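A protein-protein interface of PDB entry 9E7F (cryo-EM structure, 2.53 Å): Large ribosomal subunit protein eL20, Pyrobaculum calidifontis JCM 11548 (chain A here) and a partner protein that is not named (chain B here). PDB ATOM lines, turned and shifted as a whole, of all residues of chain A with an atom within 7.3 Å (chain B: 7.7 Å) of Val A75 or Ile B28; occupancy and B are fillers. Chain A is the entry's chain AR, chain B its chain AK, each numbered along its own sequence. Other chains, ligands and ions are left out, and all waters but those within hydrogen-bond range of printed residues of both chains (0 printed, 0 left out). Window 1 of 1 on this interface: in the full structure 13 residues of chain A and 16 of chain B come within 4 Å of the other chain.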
ATOM      1  N   PRO A   2       2.541  10.452  21.085  1.00  0.00           N
ATOM      2  CA  PRO A   2       1.801   9.863  19.972  1.00  0.00           C
ATOM      3  C   PRO A   2       2.382  10.232  18.614  1.00  0.00           C
ATOM      4  O   PRO A   2       2.586  11.406  18.319  1.00  0.00           O
ATOM      5  CB  PRO A   2       0.402  10.454  20.151  1.00  0.00           C
ATOM      6  CG  PRO A   2       0.319  10.831  21.636  1.00  0.00           C
ATOM      7  CD  PRO A   2       1.673  10.599  22.259  1.00  0.00           C
ATOM      8  N   VAL A  22      -1.076   5.021  15.021  1.00  0.00           N
ATOM      9  CA  VAL A  22      -0.740   6.096  15.943  1.00  0.00           C
ATOM     10  C   VAL A  22      -0.446   5.462  17.295  1.00  0.00           C
ATOM     11  O   VAL A  22      -1.356   4.988  17.978  1.00  0.00           O
ATOM     12  CB  VAL A  22      -1.868   7.130  16.040  1.00  0.00           C
ATOM     13  CG1 VAL A  22      -1.472   8.260  16.968  1.00  0.00           C
ATOM     14  CG2 VAL A  22      -2.203   7.661  14.660  1.00  0.00           C
ATOM     15  N   LEU A  69      -6.695  11.018  14.843  1.00  0.00           N
ATOM     16  CA  LEU A  69      -6.365  10.553  16.186  1.00  0.00           C
ATOM     17  C   LEU A  69      -5.238  11.360  16.808  1.00  0.00           C
ATOM     18  O   LEU A  69      -5.156  11.455  18.037  1.00  0.00           O
ATOM     19  CB  LEU A  69      -5.992   9.072  16.165  1.00  0.00           C
ATOM     20  CG  LEU A  69      -7.102   8.081  15.841  1.00  0.00           C
ATOM     21  CD1 LEU A  69      -6.520   6.695  15.705  1.00  0.00           C
ATOM     22  CD2 LEU A  69      -8.159   8.108  16.917  1.00  0.00           C
ATOM     23  N   MET A  70      -4.357  11.934  15.989  1.00  0.00           N
ATOM     24  CA  MET A  70      -3.234  12.688  16.535  1.00  0.00           C
ATOM     25  C   MET A  70      -3.704  13.956  17.236  1.00  0.00           C
ATOM     26  O   MET A  70      -3.156  14.339  18.275  1.00  0.00           O
ATOM     27  CB  MET A  70      -2.240  13.024  15.430  1.00  0.00           C
ATOM     28  CG  MET A  70      -1.384  11.852  14.996  1.00  0.00           C
ATOM     29  SD  MET A  70       0.244  11.866  15.767  1.00  0.00           S
ATOM     30  CE  MET A  70       0.742  13.561  15.486  1.00  0.00           C
ATOM     31  N   VAL A  71      -4.721  14.618  16.688  1.00  0.00           N
ATOM     32  CA  VAL A  71      -5.220  15.869  17.245  1.00  0.00           C
ATOM     33  C   VAL A  71      -6.426  15.653  18.155  1.00  0.00           C
ATOM     34  O   VAL A  71      -7.104  16.617  18.517  1.00  0.00           O
ATOM     35  CB  VAL A  71      -5.547  16.874  16.130  1.00  0.00           C
ATOM     36  CG1 VAL A  71      -4.322  17.124  15.285  1.00  0.00           C
ATOM     37  CG2 VAL A  71      -6.681  16.364  15.274  1.00  0.00           C
ATOM     38  N   LEU A  72      -6.706  14.410  18.531  1.00  0.00           N
ATOM     39  CA  LEU A  72      -7.827  14.126  19.415  1.00  0.00           C
ATOM     40  C   LEU A  72      -7.595  14.753  20.781  1.00  0.00           C
ATOM     41  O   LEU A  72      -6.538  14.577  21.390  1.00  0.00           O
ATOM     42  CB  LEU A  72      -8.014  12.617  19.551  1.00  0.00           C
ATOM     43  CG  LEU A  72      -9.448  12.115  19.670  1.00  0.00           C
ATOM     44  CD1 LEU A  72     -10.212  12.343  18.388  1.00  0.00           C
ATOM     45  CD2 LEU A  72      -9.445  10.645  20.045  1.00  0.00           C
ATOM     46  N   GLU A  73      -8.590  15.493  21.260  1.00  0.00           N
ATOM     47  CA  GLU A  73      -8.452  16.255  22.487  1.00  0.00           C
ATOM     48  C   GLU A  73      -9.204  15.654  23.659  1.00  0.00           C
ATOM     49  O   GLU A  73      -9.008  16.107  24.790  1.00  0.00           O
ATOM     50  CB  GLU A  73      -8.930  17.698  22.265  1.00  0.00           C
ATOM     51  CG  GLU A  73      -8.294  18.367  21.053  1.00  0.00           C
ATOM     52  CD  GLU A  73      -6.931  18.954  21.355  1.00  0.00           C
ATOM     53  OE1 GLU A  73      -6.770  19.580  22.421  1.00  0.00           O
ATOM     54  OE2 GLU A  73      -6.015  18.773  20.528  1.00  0.00           O
ATOM     55  N   LYS A  74     -10.046  14.651  23.425  1.00  0.00           N
ATOM     56  CA  LYS A  74     -10.822  14.049  24.497  1.00  0.00           C
ATOM     57  C   LYS A  74     -11.499  12.798  23.959  1.00  0.00           C
ATOM     58  O   LYS A  74     -11.800  12.701  22.766  1.00  0.00           O
ATOM     59  CB  LYS A  74     -11.817  15.064  25.075  1.00  0.00           C
ATOM     60  CG  LYS A  74     -13.205  15.089  24.482  1.00  0.00           C
ATOM     61  CD  LYS A  74     -14.165  14.235  25.287  1.00  0.00           C
ATOM     62  CE  LYS A  74     -15.478  14.069  24.563  1.00  0.00           C
ATOM     63  NZ  LYS A  74     -16.271  12.947  25.098  1.00  0.00           N
ATOM     64  N   VAL A  75     -11.727  11.832  24.854  1.00  0.00           N
ATOM     65  CA  VAL A  75     -12.129  10.488  24.463  1.00  0.00           C
ATOM     66  C   VAL A  75     -13.411  10.109  25.196  1.00  0.00           C
ATOM     67  O   VAL A  75     -13.786  10.720  26.197  1.00  0.00           O
ATOM     68  CB  VAL A  75     -11.014   9.459  24.750  1.00  0.00           C
ATOM     69  CG1 VAL A  75     -11.179   8.228  23.894  1.00  0.00           C
ATOM     70  CG2 VAL A  75      -9.660  10.076  24.531  1.00  0.00           C
ATOM     71  N   VAL A  76     -14.081   9.076  24.685  1.00  0.00           N
ATOM     72  CA  VAL A  76     -15.359   8.613  25.215  1.00  0.00           C
ATOM     73  C   VAL A  76     -15.239   7.131  25.549  1.00  0.00           C
ATOM     74  O   VAL A  76     -14.478   6.399  24.904  1.00  0.00           O
ATOM     75  CB  VAL A  76     -16.507   8.831  24.204  1.00  0.00           C
ATOM     76  CG1 VAL A  76     -17.865   8.543  24.840  1.00  0.00           C
ATOM     77  CG2 VAL A  76     -16.451  10.214  23.586  1.00  0.00           C
ATOM     78  N   ARG A  77     -15.984   6.689  26.555  1.00  0.00           N
ATOM     79  CA  ARG A  77     -16.101   5.265  26.846  1.00  0.00           C
ATOM     80  C   ARG A  77     -17.372   4.984  27.631  1.00  0.00           C
ATOM     81  O   ARG A  77     -18.432   5.521  27.317  1.00  0.00           O
ATOM     82  CB  ARG A  77     -14.882   4.761  27.613  1.00  0.00           C
ATOM     83  CG  ARG A  77     -14.521   3.314  27.318  1.00  0.00           C
ATOM     84  CD  ARG A  77     -14.171   3.124  25.850  1.00  0.00           C
ATOM     85  NE  ARG A  77     -13.240   2.021  25.640  1.00  0.00           N
ATOM     86  CZ  ARG A  77     -11.961   2.048  25.987  1.00  0.00           C
ATOM     87  NH1 ARG A  77     -11.422   3.113  26.555  1.00  0.00           N
ATOM     88  NH2 ARG A  77     -11.203   0.980  25.760  1.00  0.00           N
ATOM     89  N   VAL B   2     -21.517   7.400  30.356  1.00  0.00           N
ATOM     90  CA  VAL B   2     -20.569   7.803  29.325  1.00  0.00           C
ATOM     91  C   VAL B   2     -19.443   8.618  29.961  1.00  0.00           C
ATOM     92  O   VAL B   2     -19.672   9.648  30.591  1.00  0.00           O
ATOM     93  CB  VAL B   2     -21.288   8.564  28.185  1.00  0.00           C
ATOM     94  CG1 VAL B   2     -21.949   9.839  28.696  1.00  0.00           C
ATOM     95  CG2 VAL B   2     -20.324   8.867  27.051  1.00  0.00           C
ATOM     96  N   LYS B   3     -18.219   8.124  29.814  1.00  0.00           N
ATOM     97  CA  LYS B   3     -17.061   8.699  30.482  1.00  0.00           C
ATOM     98  C   LYS B   3     -16.336   9.646  29.541  1.00  0.00           C
ATOM     99  O   LYS B   3     -16.178   9.359  28.351  1.00  0.00           O
ATOM    100  CB  LYS B   3     -16.119   7.589  30.953  1.00  0.00           C
ATOM    101  CG  LYS B   3     -14.679   8.012  31.154  1.00  0.00           C
ATOM    102  CD  LYS B   3     -13.797   6.816  31.484  1.00  0.00           C
ATOM    103  CE  LYS B   3     -14.543   5.786  32.318  1.00  0.00           C
ATOM    104  NZ  LYS B   3     -13.638   4.747  32.886  1.00  0.00           N
ATOM    105  N   VAL B   4     -15.906  10.785  30.072  1.00  0.00           N
ATOM    106  CA  VAL B   4     -15.201  11.793  29.292  1.00  0.00           C
ATOM    107  C   VAL B   4     -13.815  11.982  29.889  1.00  0.00           C
ATOM    108  O   VAL B   4     -13.681  12.395  31.047  1.00  0.00           O
ATOM    109  CB  VAL B   4     -15.962  13.127  29.252  1.00  0.00           C
ATOM    110  CG1 VAL B   4     -14.999  14.277  29.044  1.00  0.00           C
ATOM    111  CG2 VAL B   4     -17.007  13.109  28.156  1.00  0.00           C
ATOM    112  N   ILE B   5     -12.791  11.688  29.097  1.00  0.00           N
ATOM    113  CA  ILE B   5     -11.406  11.993  29.427  1.00  0.00           C
ATOM    114  C   ILE B   5     -10.939  13.083  28.476  1.00  0.00           C
ATOM    115  O   ILE B   5     -11.066  12.942  27.255  1.00  0.00           O
ATOM    116  CB  ILE B   5     -10.514  10.748  29.312  1.00  0.00           C
ATOM    117  CG1 ILE B   5     -11.103   9.596  30.125  1.00  0.00           C
ATOM    118  CG2 ILE B   5      -9.104  11.065  29.761  1.00  0.00           C
ATOM    119  CD1 ILE B   5     -11.131   9.844  31.610  1.00  0.00           C
ATOM    120  N   ASP B   6     -10.406  14.168  29.032  1.00  0.00           N
ATOM    121  CA  ASP B   6      -9.972  15.313  28.243  1.00  0.00           C
ATOM    122  C   ASP B   6      -8.583  15.738  28.692  1.00  0.00           C
ATOM    123  O   ASP B   6      -8.179  15.482  29.827  1.00  0.00           O
ATOM    124  CB  ASP B   6     -10.998  16.462  28.339  1.00  0.00           C
ATOM    125  CG  ASP B   6     -11.151  17.027  29.752  1.00  0.00           C
ATOM    126  OD1 ASP B   6     -12.281  16.966  30.277  1.00  0.00           O
ATOM    127  OD2 ASP B   6     -10.192  17.590  30.322  1.00  0.00           O
ATOM    128  N   VAL B   7      -7.850  16.387  27.786  1.00  0.00           N
ATOM    129  CA  VAL B   7      -6.488  16.799  28.097  1.00  0.00           C
ATOM    130  C   VAL B   7      -6.520  17.871  29.175  1.00  0.00           C
ATOM    131  O   VAL B   7      -7.234  18.873  29.060  1.00  0.00           O
ATOM    132  CB  VAL B   7      -5.774  17.290  26.831  1.00  0.00           C
ATOM    133  CG1 VAL B   7      -4.496  17.995  27.194  1.00  0.00           C
ATOM    134  CG2 VAL B   7      -5.486  16.129  25.905  1.00  0.00           C
ATOM    135  N   GLY B   8      -5.745  17.657  30.234  1.00  0.00           N
ATOM    136  CA  GLY B   8      -5.777  18.518  31.395  1.00  0.00           C
ATOM    137  C   GLY B   8      -6.760  18.100  32.461  1.00  0.00           C
ATOM    138  O   GLY B   8      -6.792  18.722  33.528  1.00  0.00           O
ATOM    139  N   VAL B  25      -4.170  14.290  32.846  1.00  0.00           N
ATOM    140  CA  VAL B  25      -4.096  13.889  31.446  1.00  0.00           C
ATOM    141  C   VAL B  25      -3.319  14.949  30.682  1.00  0.00           C
ATOM    142  O   VAL B  25      -3.640  16.139  30.753  1.00  0.00           O
ATOM    143  CB  VAL B  25      -5.497  13.701  30.854  1.00  0.00           C
ATOM    144  CG1 VAL B  25      -5.406  13.242  29.413  1.00  0.00           C
ATOM    145  CG2 VAL B  25      -6.298  12.722  31.689  1.00  0.00           C
ATOM    146  N   VAL B  26      -2.296  14.524  29.948  1.00  0.00           N
ATOM    147  CA  VAL B  26      -1.483  15.453  29.179  1.00  0.00           C
ATOM    148  C   VAL B  26      -1.495  15.162  27.688  1.00  0.00           C
ATOM    149  O   VAL B  26      -1.084  16.030  26.902  1.00  0.00           O
ATOM    150  CB  VAL B  26      -0.032  15.493  29.699  1.00  0.00           C
ATOM    151  CG1 VAL B  26       0.056  16.361  30.930  1.00  0.00           C
ATOM    152  CG2 VAL B  26       0.472  14.097  29.987  1.00  0.00           C
ATOM    153  N   ASP B  27      -1.933  13.985  27.255  1.00  0.00           N
ATOM    154  CA  ASP B  27      -2.034  13.718  25.829  1.00  0.00           C
ATOM    155  C   ASP B  27      -2.923  12.506  25.624  1.00  0.00           C
ATOM    156  O   ASP B  27      -3.134  11.706  26.536  1.00  0.00           O
ATOM    157  CB  ASP B  27      -0.660  13.501  25.192  1.00  0.00           C
ATOM    158  CG  ASP B  27      -0.576  14.061  23.779  1.00  0.00           C
ATOM    159  OD1 ASP B  27      -1.634  14.409  23.211  1.00  0.00           O
ATOM    160  OD2 ASP B  27       0.544  14.157  23.233  1.00  0.00           O
ATOM    161  N   ILE B  28      -3.444  12.385  24.409  1.00  0.00           N
ATOM    162  CA  ILE B  28      -4.297  11.272  24.017  1.00  0.00           C
ATOM    163  C   ILE B  28      -3.562  10.475  22.954  1.00  0.00           C
ATOM    164  O   ILE B  28      -3.290  10.989  21.863  1.00  0.00           O
ATOM    165  CB  ILE B  28      -5.657  11.750  23.494  1.00  0.00           C
ATOM    166  CG1 ILE B  28      -6.250  12.796  24.434  1.00  0.00           C
ATOM    167  CG2 ILE B  28      -6.592  10.577  23.323  1.00  0.00           C
ATOM    168  CD1 ILE B  28      -7.095  12.217  25.534  1.00  0.00           C
ATOM    169  N   VAL B  29      -3.249   9.220  23.268  1.00  0.00           N
ATOM    170  CA  VAL B  29      -2.556   8.362  22.313  1.00  0.00           C
ATOM    171  C   VAL B  29      -3.503   7.926  21.206  1.00  0.00           C
ATOM    172  O   VAL B  29      -3.273   8.189  20.021  1.00  0.00           O
ATOM    173  CB  VAL B  29      -1.942   7.148  23.032  1.00  0.00           C
ATOM    174  CG1 VAL B  29      -1.242   6.249  22.037  1.00  0.00           C
ATOM    175  CG2 VAL B  29      -0.987   7.597  24.125  1.00  0.00           C
ATOM    176  N   ASP B  30      -4.587   7.260  21.584  1.00  0.00           N
ATOM    177  CA  ASP B  30      -5.599   6.778  20.658  1.00  0.00           C
ATOM    178  C   ASP B  30      -6.958   6.950  21.322  1.00  0.00           C
ATOM    179  O   ASP B  30      -7.101   7.687  22.299  1.00  0.00           O
ATOM    180  CB  ASP B  30      -5.278   5.342  20.210  1.00  0.00           C
ATOM    181  CG  ASP B  30      -5.317   4.311  21.349  1.00  0.00           C
ATOM    182  OD1 ASP B  30      -5.599   4.640  22.521  1.00  0.00           O
ATOM    183  OD2 ASP B  30      -5.062   3.128  21.053  1.00  0.00           O
ATOM    184  N   GLU B  31      -7.970   6.262  20.796  1.00  0.00           N
ATOM    185  CA  GLU B  31      -9.270   6.301  21.452  1.00  0.00           C
ATOM    186  C   GLU B  31      -9.336   5.389  22.673  1.00  0.00           C
ATOM    187  O   GLU B  31     -10.361   5.375  23.360  1.00  0.00           O
ATOM    188  CB  GLU B  31     -10.376   5.935  20.464  1.00  0.00           C
ATOM    189  CG  GLU B  31     -10.913   7.133  19.706  1.00  0.00           C
ATOM    190  CD  GLU B  31     -12.220   7.658  20.267  1.00  0.00           C
ATOM    191  OE1 GLU B  31     -13.286   7.136  19.894  1.00  0.00           O
ATOM    192  OE2 GLU B  31     -12.184   8.614  21.066  1.00  0.00           O
ATOM    193  N   ASN B  32      -8.282   4.624  22.948  1.00  0.00           N
ATOM    194  CA  ASN B  32      -8.237   3.732  24.094  1.00  0.00           C
ATOM    195  C   ASN B  32      -7.208   4.123  25.140  1.00  0.00           C
ATOM    196  O   ASN B  32      -7.376   3.776  26.308  1.00  0.00           O
ATOM    197  CB  ASN B  32      -7.945   2.302  23.632  1.00  0.00           C
ATOM    198  CG  ASN B  32      -9.035   1.741  22.757  1.00  0.00           C
ATOM    199  OD1 ASN B  32     -10.205   1.738  23.129  1.00  0.00           O
ATOM    200  ND2 ASN B  32      -8.658   1.264  21.582  1.00  0.00           N
ATOM    201  N   TYR B  33      -6.147   4.819  24.757  1.00  0.00           N
ATOM    202  CA  TYR B  33      -5.067   5.146  25.674  1.00  0.00           C
ATOM    203  C   TYR B  33      -4.831   6.646  25.690  1.00  0.00           C
ATOM    204  O   TYR B  33      -4.861   7.301  24.648  1.00  0.00           O
ATOM    205  CB  TYR B  33      -3.767   4.437  25.289  1.00  0.00           C
ATOM    206  CG  TYR B  33      -3.750   2.957  25.567  1.00  0.00           C
ATOM    207  CD1 TYR B  33      -4.319   2.058  24.685  1.00  0.00           C
ATOM    208  CD2 TYR B  33      -3.147   2.459  26.707  1.00  0.00           C
ATOM    209  CE1 TYR B  33      -4.295   0.708  24.936  1.00  0.00           C
ATOM    210  CE2 TYR B  33      -3.120   1.112  26.963  1.00  0.00           C
ATOM    211  CZ  TYR B  33      -3.696   0.242  26.075  1.00  0.00           C
ATOM    212  OH  TYR B  33      -3.672  -1.104  26.323  1.00  0.00           O
ATOM    213  N   VAL B  34      -4.587   7.179  26.883  1.00  0.00           N
ATOM    214  CA  VAL B  34      -4.194   8.564  27.071  1.00  0.00           C
ATOM    215  C   VAL B  34      -2.903   8.575  27.875  1.00  0.00           C
ATOM    216  O   VAL B  34      -2.468   7.555  28.409  1.00  0.00           O
ATOM    217  CB  VAL B  34      -5.280   9.395  27.778  1.00  0.00           C
ATOM    218  CG1 VAL B  34      -6.626   9.129  27.156  1.00  0.00           C
ATOM    219  CG2 VAL B  34      -5.310   9.075  29.248  1.00  0.00           C
ATOM    220  N   VAL B  35      -2.285   9.747  27.950  1.00  0.00           N
ATOM    221  CA  VAL B  35      -1.041   9.936  28.682  1.00  0.00           C
ATOM    222  C   VAL B  35      -1.346  10.720  29.946  1.00  0.00           C
ATOM    223  O   VAL B  35      -1.920  11.812  29.884  1.00  0.00           O
ATOM    224  CB  VAL B  35       0.017  10.652  27.829  1.00  0.00           C
ATOM    225  CG1 VAL B  35       1.310  10.767  28.598  1.00  0.00           C
ATOM    226  CG2 VAL B  35       0.238   9.896  26.537  1.00  0.00           C
ATOM    227  N   ILE B  36      -0.960  10.165  31.089  1.00  0.00           N
ATOM    228  CA  ILE B  36      -1.238  10.761  32.386  1.00  0.00           C
ATOM    229  C   ILE B  36       0.075  10.986  33.117  1.00  0.00           C
ATOM    230  O   ILE B  36       1.020  10.199  32.983  1.00  0.00           O
ATOM    231  CB  ILE B  36      -2.182   9.888  33.237  1.00  0.00           C
ATOM    232  CG1 ILE B  36      -1.407   8.745  33.884  1.00  0.00           C
ATOM    233  CG2 ILE B  36      -3.314   9.362  32.399  1.00  0.00           C
ATOM    234  CD1 ILE B  36      -2.094   8.136  35.064  1.00  0.00           C
ATOM    235  N   ILE B  52      -7.877   3.790  29.183  1.00  0.00           N
ATOM    236  CA  ILE B  52      -9.008   4.601  29.624  1.00  0.00           C
ATOM    237  C   ILE B  52      -9.891   3.823  30.588  1.00  0.00           C
ATOM    238  O   ILE B  52     -10.559   4.412  31.445  1.00  0.00           O
ATOM    239  CB  ILE B  52      -9.796   5.117  28.404  1.00  0.00           C
ATOM    240  CG1 ILE B  52      -8.932   6.090  27.602  1.00  0.00           C
ATOM    241  CG2 ILE B  52     -11.076   5.794  28.833  1.00  0.00           C
ATOM    242  CD1 ILE B  52      -9.683   6.859  26.550  1.00  0.00           C
ATOM    243  N   LYS B  66      -1.273  20.032  24.648  1.00  0.00           N
ATOM    244  CA  LYS B  66      -1.113  18.602  24.420  1.00  0.00           C
ATOM    245  C   LYS B  66       0.339  18.196  24.636  1.00  0.00           C
ATOM    246  O   LYS B  66       1.259  18.825  24.105  1.00  0.00           O
ATOM    247  CB  LYS B  66      -1.561  18.236  23.006  1.00  0.00           C
ATOM    248  CG  LYS B  66      -3.004  17.785  22.905  1.00  0.00           C
ATOM    249  CD  LYS B  66      -3.397  17.545  21.459  1.00  0.00           C
ATOM    250  CE  LYS B  66      -3.762  16.091  21.214  1.00  0.00           C
ATOM    251  NZ  LYS B  66      -2.559  15.221  21.090  1.00  0.00           N
ATOM    252  N   GLY B  67       0.542  17.130  25.401  1.00  0.00           N
ATOM    253  CA  GLY B  67       1.894  16.727  25.752  1.00  0.00           C
ATOM    254  C   GLY B  67       2.597  17.720  26.651  1.00  0.00           C
ATOM    255  O   GLY B  67       3.784  18.005  26.454  1.00  0.00           O
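O of Val A75 lies close to O of Lys B3.
N of Val B7 sits at hydrogen-bond distance from O of Glu A73, at 3.2 Å.
O of Ile B5 sits at hydrogen-bond distance from N of Val A75 (2.7 Å).
The backbone NH (N) of Arg A77 lies within hydrogen-bond range of the backbone carbonyl oxygen (O) of Lys B3 (3.2 Å).
NZ of Lys B66 lies within hydrogen-bond range of O of Met A70 (3.0 Å).
The side-chain amide oxygen (OD1) of Asn B32 lies within hydrogen-bond range of the guanidinium group (NH2) of Arg A77, at 2.9 Å.
OD1 of Asp B27 lies within salt-bridge range of NZ of Lys B66 (2.5 Å).
O of Ile B52 sits at hydrogen-bond distance from NZ of Lys B3 (3.4 Å).
The side-chain carboxylate (OD1) of Asp B30 sits at hydrogen-bond distance from the backbone NH (N) of Asn B32, at 2.7 Å.
The backbone carbonyl oxygen of Asn B32 is in hydrogen-bond range of the backbone NH of Ile B52, at 2.9 Å.
O of Asp B27 sits at hydrogen-bond distance from N of Val B35 (2.6 Å).
Asp B27 touches Pro A2.
Pro A2 touches Val B29.
O of Val B29 touches CG1 of Val A22, at 3.5 Å.
Leu A72 touches Ile B28 (O to CG1, 3.5 Å).
O of Leu A72 touches CE of Lys B66, 3.2 Å away.
Glu A73 touches Lys B66 (OE2 to CD, 3.0 Å).
O of Ile B5 touches CA of Lys A74, at 3.0 Å.
Lys A74 touches Asp B6 (CB to CB, 3.6 Å).
Val B4 touches Val A75 (CA to O, 3.6 Å).
Val A76 touches Val B2 (CG1 to CG2, 3.3 Å).
Printed residues of chain B within 4 Å of Glu A73: Asp B6 (3.7 Å), Val B7 (3.2 Å) and Lys B66 (3.0 Å).
Printed residues of chain B within 4 Å of Lys A74: Val B4, Ile B5 and Asp B6.
Of chain B, only Lys B3 (3.5 Å), Val B4 (3.6 Å), Ile B5 (2.7 Å), Ile B28 (3.3 Å), Glu B31 (3.0 Å) and Ile B52 (3.3 Å) come within 4 Å of Val A75.
Of the printed residues of chain A, Ile B28 touches Pro A2 (3.6 Å), Leu A72 (3.5 Å) and Val A75 (3.3 Å).
Asp B30 touches none of the printed residues of chain A.
Printed residues of chain A within 4 Å of Lys B66: Met A70, Leu A72 and Glu A73.
The nearest residue of chain A that does not touch Ile B28 is Glu A73 (4.2 Å).
The nearest printed residue of chain B that does not touch Arg A77 is Glu B31 (4.1 Å).
Hydrophobic or aromatic side chains of chain A that line the printed part of chain B: Pro A2, Val A22, Leu A72, Val A75 and Val A76.
Along chain A the printed residues that touch a printed residue of chain B span positions 2 to 77.
Hydrophobic or aromatic side chains of chain B that line the printed part of chain A: Val B2, Val B4, Val B7, Ile B28 and Ile B52.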
